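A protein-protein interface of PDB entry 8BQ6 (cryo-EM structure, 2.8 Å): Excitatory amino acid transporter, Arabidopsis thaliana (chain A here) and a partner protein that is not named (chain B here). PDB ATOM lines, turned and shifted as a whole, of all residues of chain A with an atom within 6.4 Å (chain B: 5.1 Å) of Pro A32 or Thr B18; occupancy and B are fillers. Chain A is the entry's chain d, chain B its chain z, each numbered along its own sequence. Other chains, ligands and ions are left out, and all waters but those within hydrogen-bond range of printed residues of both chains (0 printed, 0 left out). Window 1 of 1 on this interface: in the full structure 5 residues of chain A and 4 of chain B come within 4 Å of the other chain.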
ATOM      1  N   GLN A  17      31.457  -5.228 -13.812  1.00  0.00           N
ATOM      2  CA  GLN A  17      30.813  -6.522 -13.448  1.00  0.00           C
ATOM      3  C   GLN A  17      29.287  -6.407 -13.585  1.00  0.00           C
ATOM      4  O   GLN A  17      28.683  -7.322 -14.165  1.00  0.00           O
ATOM      5  CB  GLN A  17      31.270  -7.005 -12.067  1.00  0.00           C
ATOM      6  CG  GLN A  17      30.698  -8.353 -11.650  1.00  0.00           C
ATOM      7  CD  GLN A  17      30.845  -9.464 -12.662  1.00  0.00           C
ATOM      8  OE1 GLN A  17      31.936  -9.765 -13.140  1.00  0.00           O
ATOM      9  NE2 GLN A  17      29.733 -10.103 -12.980  1.00  0.00           N
ATOM     10  N   MET A  29      23.428  -8.125  -9.348  1.00  0.00           N
ATOM     11  CA  MET A  29      24.346  -8.609  -8.286  1.00  0.00           C
ATOM     12  C   MET A  29      24.519 -10.131  -8.316  1.00  0.00           C
ATOM     13  O   MET A  29      24.912 -10.689  -7.277  1.00  0.00           O
ATOM     14  CB  MET A  29      23.840  -8.159  -6.913  1.00  0.00           C
ATOM     15  CG  MET A  29      23.946  -6.667  -6.703  1.00  0.00           C
ATOM     16  SD  MET A  29      25.652  -6.071  -6.719  1.00  0.00           S
ATOM     17  CE  MET A  29      26.403  -7.138  -5.491  1.00  0.00           C
ATOM     18  N   ARG A  30      24.282 -10.774  -9.458  1.00  0.00           N
ATOM     19  CA  ARG A  30      24.554 -12.229  -9.585  1.00  0.00           C
ATOM     20  C   ARG A  30      26.060 -12.464  -9.391  1.00  0.00           C
ATOM     21  O   ARG A  30      26.837 -11.769 -10.062  1.00  0.00           O
ATOM     22  CB  ARG A  30      24.033 -12.718 -10.940  1.00  0.00           C
ATOM     23  CG  ARG A  30      24.376 -14.158 -11.283  1.00  0.00           C
ATOM     24  CD  ARG A  30      23.639 -15.177 -10.436  1.00  0.00           C
ATOM     25  NE  ARG A  30      22.191 -15.028 -10.401  1.00  0.00           N
ATOM     26  CZ  ARG A  30      21.343 -15.640 -11.220  1.00  0.00           C
ATOM     27  NH1 ARG A  30      21.792 -16.448 -12.166  1.00  0.00           N
ATOM     28  NH2 ARG A  30      20.045 -15.444 -11.091  1.00  0.00           N
ATOM     29  N   HIS A  31      26.448 -13.393  -8.507  1.00  0.00           N
ATOM     30  CA  HIS A  31      27.880 -13.677  -8.180  1.00  0.00           C
ATOM     31  C   HIS A  31      28.590 -12.427  -7.613  1.00  0.00           C
ATOM     32  O   HIS A  31      29.498 -11.928  -8.275  1.00  0.00           O
ATOM     33  CB  HIS A  31      28.585 -14.339  -9.376  1.00  0.00           C
ATOM     34  CG  HIS A  31      28.009 -15.645  -9.807  1.00  0.00           C
ATOM     35  ND1 HIS A  31      28.547 -16.370 -10.847  1.00  0.00           N
ATOM     36  CD2 HIS A  31      26.964 -16.365  -9.349  1.00  0.00           C
ATOM     37  CE1 HIS A  31      27.856 -17.478 -11.014  1.00  0.00           C
ATOM     38  NE2 HIS A  31      26.878 -17.497 -10.110  1.00  0.00           N
ATOM     39  N   PRO A  32      28.236 -11.933  -6.399  1.00  0.00           N
ATOM     40  CA  PRO A  32      28.831 -10.738  -5.761  1.00  0.00           C
ATOM     41  C   PRO A  32      30.334 -10.825  -5.521  1.00  0.00           C
ATOM     42  O   PRO A  32      31.026  -9.790  -5.526  1.00  0.00           O
ATOM     43  CB  PRO A  32      28.056 -10.629  -4.441  1.00  0.00           C
ATOM     44  CG  PRO A  32      27.479 -11.985  -4.210  1.00  0.00           C
ATOM     45  CD  PRO A  32      27.207 -12.563  -5.556  1.00  0.00           C
ATOM     46  N   TRP A  33      30.866 -12.028  -5.303  1.00  0.00           N
ATOM     47  CA  TRP A  33      32.310 -12.156  -5.166  1.00  0.00           C
ATOM     48  C   TRP A  33      33.025 -11.685  -6.429  1.00  0.00           C
ATOM     49  O   TRP A  33      34.129 -11.130  -6.350  1.00  0.00           O
ATOM     50  CB  TRP A  33      32.677 -13.601  -4.816  1.00  0.00           C
ATOM     51  CG  TRP A  33      32.214 -14.614  -5.809  1.00  0.00           C
ATOM     52  CD1 TRP A  33      32.882 -15.026  -6.919  1.00  0.00           C
ATOM     53  CD2 TRP A  33      30.986 -15.356  -5.780  1.00  0.00           C
ATOM     54  NE1 TRP A  33      32.150 -15.971  -7.590  1.00  0.00           N
ATOM     55  CE2 TRP A  33      30.982 -16.194  -6.912  1.00  0.00           C
ATOM     56  CE3 TRP A  33      29.891 -15.389  -4.913  1.00  0.00           C
ATOM     57  CZ2 TRP A  33      29.925 -17.054  -7.200  1.00  0.00           C
ATOM     58  CZ3 TRP A  33      28.845 -16.244  -5.200  1.00  0.00           C
ATOM     59  CH2 TRP A  33      28.868 -17.063  -6.336  1.00  0.00           C
ATOM     60  N   GLU A  34      32.401 -11.865  -7.597  1.00  0.00           N
ATOM     61  CA  GLU A  34      32.959 -11.310  -8.826  1.00  0.00           C
ATOM     62  C   GLU A  34      32.952  -9.790  -8.808  1.00  0.00           C
ATOM     63  O   GLU A  34      33.840  -9.165  -9.389  1.00  0.00           O
ATOM     64  CB  GLU A  34      32.192 -11.809 -10.046  1.00  0.00           C
ATOM     65  CG  GLU A  34      32.199 -13.306 -10.212  1.00  0.00           C
ATOM     66  CD  GLU A  34      31.340 -13.755 -11.370  1.00  0.00           C
ATOM     67  OE1 GLU A  34      30.703 -12.895 -12.010  1.00  0.00           O
ATOM     68  OE2 GLU A  34      31.288 -14.971 -11.632  1.00  0.00           O
ATOM     69  N   HIS A  35      31.971  -9.192  -8.133  1.00  0.00           N
ATOM     70  CA  HIS A  35      31.925  -7.713  -8.003  1.00  0.00           C
ATOM     71  C   HIS A  35      33.116  -7.264  -7.157  1.00  0.00           C
ATOM     72  O   HIS A  35      33.700  -6.225  -7.485  1.00  0.00           O
ATOM     73  CB  HIS A  35      30.581  -7.251  -7.429  1.00  0.00           C
ATOM     74  CG  HIS A  35      29.418  -7.534  -8.312  1.00  0.00           C
ATOM     75  ND1 HIS A  35      28.924  -8.804  -8.499  1.00  0.00           N
ATOM     76  CD2 HIS A  35      28.654  -6.716  -9.063  1.00  0.00           C
ATOM     77  CE1 HIS A  35      27.904  -8.760  -9.323  1.00  0.00           C
ATOM     78  NE2 HIS A  35      27.725  -7.493  -9.686  1.00  0.00           N
ATOM     79  N   VAL A  36      33.463  -8.033  -6.123  1.00  0.00           N
ATOM     80  CA  VAL A  36      34.630  -7.710  -5.302  1.00  0.00           C
ATOM     81  C   VAL A  36      35.915  -7.843  -6.118  1.00  0.00           C
ATOM     82  O   VAL A  36      36.808  -6.977  -6.075  1.00  0.00           O
ATOM     83  CB  VAL A  36      34.650  -8.606  -4.052  1.00  0.00           C
ATOM     84  CG1 VAL A  36      35.874  -8.334  -3.210  1.00  0.00           C
ATOM     85  CG2 VAL A  36      33.380  -8.392  -3.247  1.00  0.00           C
ATOM     86  N   VAL A  37      36.021  -8.933  -6.884  1.00  0.00           N
ATOM     87  CA  VAL A  37      37.190  -9.159  -7.730  1.00  0.00           C
ATOM     88  C   VAL A  37      37.342  -8.035  -8.748  1.00  0.00           C
ATOM     89  O   VAL A  37      38.452  -7.548  -9.002  1.00  0.00           O
ATOM     90  CB  VAL A  37      37.076 -10.532  -8.419  1.00  0.00           C
ATOM     91  CG1 VAL A  37      37.941 -10.585  -9.669  1.00  0.00           C
ATOM     92  CG2 VAL A  37      37.442 -11.637  -7.454  1.00  0.00           C
ATOM     93  N   PHE B  13      20.520 -11.815   0.862  1.00  0.00           N
ATOM     94  CA  PHE B  13      20.571 -12.773  -0.277  1.00  0.00           C
ATOM     95  C   PHE B  13      21.978 -12.834  -0.893  1.00  0.00           C
ATOM     96  O   PHE B  13      22.340 -13.914  -1.350  1.00  0.00           O
ATOM     97  CB  PHE B  13      19.524 -12.391  -1.326  1.00  0.00           C
ATOM     98  CG  PHE B  13      18.241 -13.177  -1.285  1.00  0.00           C
ATOM     99  CD1 PHE B  13      18.237 -14.518  -0.938  1.00  0.00           C
ATOM    100  CD2 PHE B  13      17.034 -12.575  -1.597  1.00  0.00           C
ATOM    101  CE1 PHE B  13      17.053 -15.238  -0.902  1.00  0.00           C
ATOM    102  CE2 PHE B  13      15.851 -13.293  -1.557  1.00  0.00           C
ATOM    103  CZ  PHE B  13      15.863 -14.624  -1.212  1.00  0.00           C
ATOM    104  N   TRP B  14      22.725 -11.721  -0.916  1.00  0.00           N
ATOM    105  CA  TRP B  14      24.125 -11.716  -1.430  1.00  0.00           C
ATOM    106  C   TRP B  14      25.003 -12.594  -0.535  1.00  0.00           C
ATOM    107  O   TRP B  14      25.760 -13.404  -1.086  1.00  0.00           O
ATOM    108  CB  TRP B  14      24.711 -10.304  -1.504  1.00  0.00           C
ATOM    109  CG  TRP B  14      23.925  -9.264  -2.237  1.00  0.00           C
ATOM    110  CD1 TRP B  14      22.882  -9.439  -3.098  1.00  0.00           C
ATOM    111  CD2 TRP B  14      24.162  -7.849  -2.178  1.00  0.00           C
ATOM    112  NE1 TRP B  14      22.441  -8.229  -3.559  1.00  0.00           N
ATOM    113  CE2 TRP B  14      23.208  -7.235  -3.014  1.00  0.00           C
ATOM    114  CE3 TRP B  14      25.080  -7.045  -1.495  1.00  0.00           C
ATOM    115  CZ2 TRP B  14      23.152  -5.852  -3.183  1.00  0.00           C
ATOM    116  CZ3 TRP B  14      25.025  -5.681  -1.664  1.00  0.00           C
ATOM    117  CH2 TRP B  14      24.073  -5.095  -2.498  1.00  0.00           C
ATOM    118  N   ILE B  15      24.906 -12.423   0.787  1.00  0.00           N
ATOM    119  CA  ILE B  15      25.689 -13.258   1.748  1.00  0.00           C
ATOM    120  C   ILE B  15      25.306 -14.732   1.584  1.00  0.00           C
ATOM    121  O   ILE B  15      26.215 -15.574   1.601  1.00  0.00           O
ATOM    122  CB  ILE B  15      25.491 -12.765   3.196  1.00  0.00           C
ATOM    123  CG1 ILE B  15      25.602 -11.243   3.299  1.00  0.00           C
ATOM    124  CG2 ILE B  15      26.452 -13.461   4.147  1.00  0.00           C
ATOM    125  CD1 ILE B  15      25.808 -10.738   4.704  1.00  0.00           C
ATOM    126  N   ARG B  16      24.012 -15.026   1.468  1.00  0.00           N
ATOM    127  CA  ARG B  16      23.526 -16.417   1.297  1.00  0.00           C
ATOM    128  C   ARG B  16      24.051 -16.990  -0.021  1.00  0.00           C
ATOM    129  O   ARG B  16      24.588 -18.094   0.017  1.00  0.00           O
ATOM    130  CB  ARG B  16      21.999 -16.408   1.322  1.00  0.00           C
ATOM    131  CG  ARG B  16      21.399 -16.000   2.657  1.00  0.00           C
ATOM    132  CD  ARG B  16      19.944 -16.394   2.734  1.00  0.00           C
ATOM    133  NE  ARG B  16      19.812 -17.842   2.715  1.00  0.00           N
ATOM    134  CZ  ARG B  16      18.695 -18.501   2.991  1.00  0.00           C
ATOM    135  NH1 ARG B  16      17.599 -17.839   3.322  1.00  0.00           N
ATOM    136  NH2 ARG B  16      18.682 -19.821   2.945  1.00  0.00           N
ATOM    137  N   GLU B  17      23.895 -16.257  -1.131  1.00  0.00           N
ATOM    138  CA  GLU B  17      24.435 -16.693  -2.448  1.00  0.00           C
ATOM    139  C   GLU B  17      25.915 -17.050  -2.295  1.00  0.00           C
ATOM    140  O   GLU B  17      26.307 -18.113  -2.787  1.00  0.00           O
ATOM    141  CB  GLU B  17      24.256 -15.598  -3.501  1.00  0.00           C
ATOM    142  CG  GLU B  17      24.864 -15.950  -4.848  1.00  0.00           C
ATOM    143  CD  GLU B  17      24.190 -15.380  -6.084  1.00  0.00           C
ATOM    144  OE1 GLU B  17      23.432 -14.403  -5.956  1.00  0.00           O
ATOM    145  OE2 GLU B  17      24.435 -15.917  -7.177  1.00  0.00           O
ATOM    146  N   THR B  18      26.691 -16.191  -1.619  1.00  0.00           N
ATOM    147  CA  THR B  18      28.117 -16.455  -1.435  1.00  0.00           C
ATOM    148  C   THR B  18      28.356 -17.710  -0.598  1.00  0.00           C
ATOM    149  O   THR B  18      29.212 -18.539  -0.937  1.00  0.00           O
ATOM    150  CB  THR B  18      28.789 -15.244  -0.792  1.00  0.00           C
ATOM    151  OG1 THR B  18      28.602 -14.100  -1.630  1.00  0.00           O
ATOM    152  CG2 THR B  18      30.271 -15.489  -0.610  1.00  0.00           C
ATOM    153  N   GLY B  19      27.607 -17.871   0.494  1.00  0.00           N
ATOM    154  CA  GLY B  19      27.794 -19.042   1.339  1.00  0.00           C
ATOM    155  C   GLY B  19      27.443 -20.343   0.640  1.00  0.00           C
ATOM    156  O   GLY B  19      28.144 -21.350   0.784  1.00  0.00           O
ATOM    157  N   GLN B  20      26.351 -20.346  -0.121  1.00  0.00           N
ATOM    158  CA  GLN B  20      25.970 -21.564  -0.826  1.00  0.00           C
ATOM    159  C   GLN B  20      26.968 -21.895  -1.928  1.00  0.00           C
ATOM    160  O   GLN B  20      27.273 -23.072  -2.167  1.00  0.00           O
ATOM    161  CB  GLN B  20      24.560 -21.423  -1.384  1.00  0.00           C
ATOM    162  CG  GLN B  20      23.499 -21.589  -0.328  1.00  0.00           C
ATOM    163  CD  GLN B  20      22.135 -21.198  -0.822  1.00  0.00           C
ATOM    164  OE1 GLN B  20      21.747 -21.542  -1.935  1.00  0.00           O
ATOM    165  NE2 GLN B  20      21.391 -20.480   0.006  1.00  0.00           N
ATOM    166  N   ALA B  21      27.507 -20.867  -2.591  1.00  0.00           N
ATOM    167  CA  ALA B  21      28.576 -21.093  -3.555  1.00  0.00           C
ATOM    168  C   ALA B  21      29.793 -21.725  -2.890  1.00  0.00           C
ATOM    169  O   ALA B  21      30.418 -22.635  -3.453  1.00  0.00           O
ATOM    170  CB  ALA B  21      28.957 -19.774  -4.224  1.00  0.00           C
ATOM    171  N   LEU B  22      30.150 -21.244  -1.694  1.00  0.00           N
ATOM    172  CA  LEU B  22      31.273 -21.825  -0.959  1.00  0.00           C
ATOM    173  C   LEU B  22      31.016 -23.283  -0.604  1.00  0.00           C
ATOM    174  O   LEU B  22      31.923 -24.123  -0.686  1.00  0.00           O
ATOM    175  CB  LEU B  22      31.536 -21.027   0.314  1.00  0.00           C
ATOM    176  CG  LEU B  22      32.646 -19.985   0.291  1.00  0.00           C
ATOM    177  CD1 LEU B  22      32.789 -19.376   1.672  1.00  0.00           C
ATOM    178  CD2 LEU B  22      33.939 -20.629  -0.154  1.00  0.00           C
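NE1 of Trp B14 touches CB of Met A29, at 3.6 Å.
Glu B17 touches Arg A30.
Pro A32 touches Trp B14 (CG to O, 3.8 Å).
Thr B18 touches Pro A32 (OG1 to CG, 3.5 Å).
Glu B17 touches Trp A33 (O to CZ3, 3.97 Å).
Trp A33 touches Thr B18 (CE3 to OG1, 3.8 Å).
CH2 of Trp A33 touches CB of Ala B21, at 3.4 Å.
Printed residues of chain A that touch a printed residue of chain B: Met A29, Arg A30, His A31, Pro A32 and Trp A33.
Hydrophobic or aromatic side chains of chain A that line the printed part of chain B: Met A29, His A31, Pro A32 and Trp A33.
Of the 10 printed residues of chain B, 4 touch a printed residue of chain A.
Printed residues of chain B that touch a printed residue of chain A: Trp B14, Glu B17, Thr B18 and Ala B21.
Hydrophobic or aromatic side chains of chain B that line the printed part of chain A: Trp B14 and Ala B21.
Among the printed residues, 8 pairs touch across the chains.
Among the printed residues, no Asp or Glu carboxylate lies within 4 Å of a Lys or Arg side-chain nitrogen of the other chain.
A ring nitrogen (ND1) of His A31 lies within hydrogen-bond range of the side-chain carboxylate of Glu A34, 3.2 Å away.
The backbone carbonyl oxygen (O) of His A31 sits at hydrogen-bond distance from a ring nitrogen (ND1) of His A35.
OG1 of Thr B18 is in hydrogen-bond range of O of Trp B14, at 3.0 Å.
OE2 of Glu B17 sits close to N of His A31, at 3.5 Å.
Of the printed residues of chain B, Met A29 touches Trp B14 (3.6 Å).
Of the printed residues of chain A, Glu B17 touches Arg A30 (3.4 Å), His A31 (3.4 Å) and Trp A33 (3.97 Å).
Of the printed residues of chain B, His A31 touches Glu B17 (3.4 Å).
Printed residues of chain A within 4 Å of Ala B21: Trp A33 (3.4 Å).
Printed residues of chain B within 4 Å of Trp A33: Glu B17, Thr B18 and Ala B21.
Glu A34 touches none of the printed residues of chain B.
Arg B16 touches none of the printed residues of chain A.
The nearest residue of chain B that does not touch Pro A32 is Glu B17 (4.2 Å).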
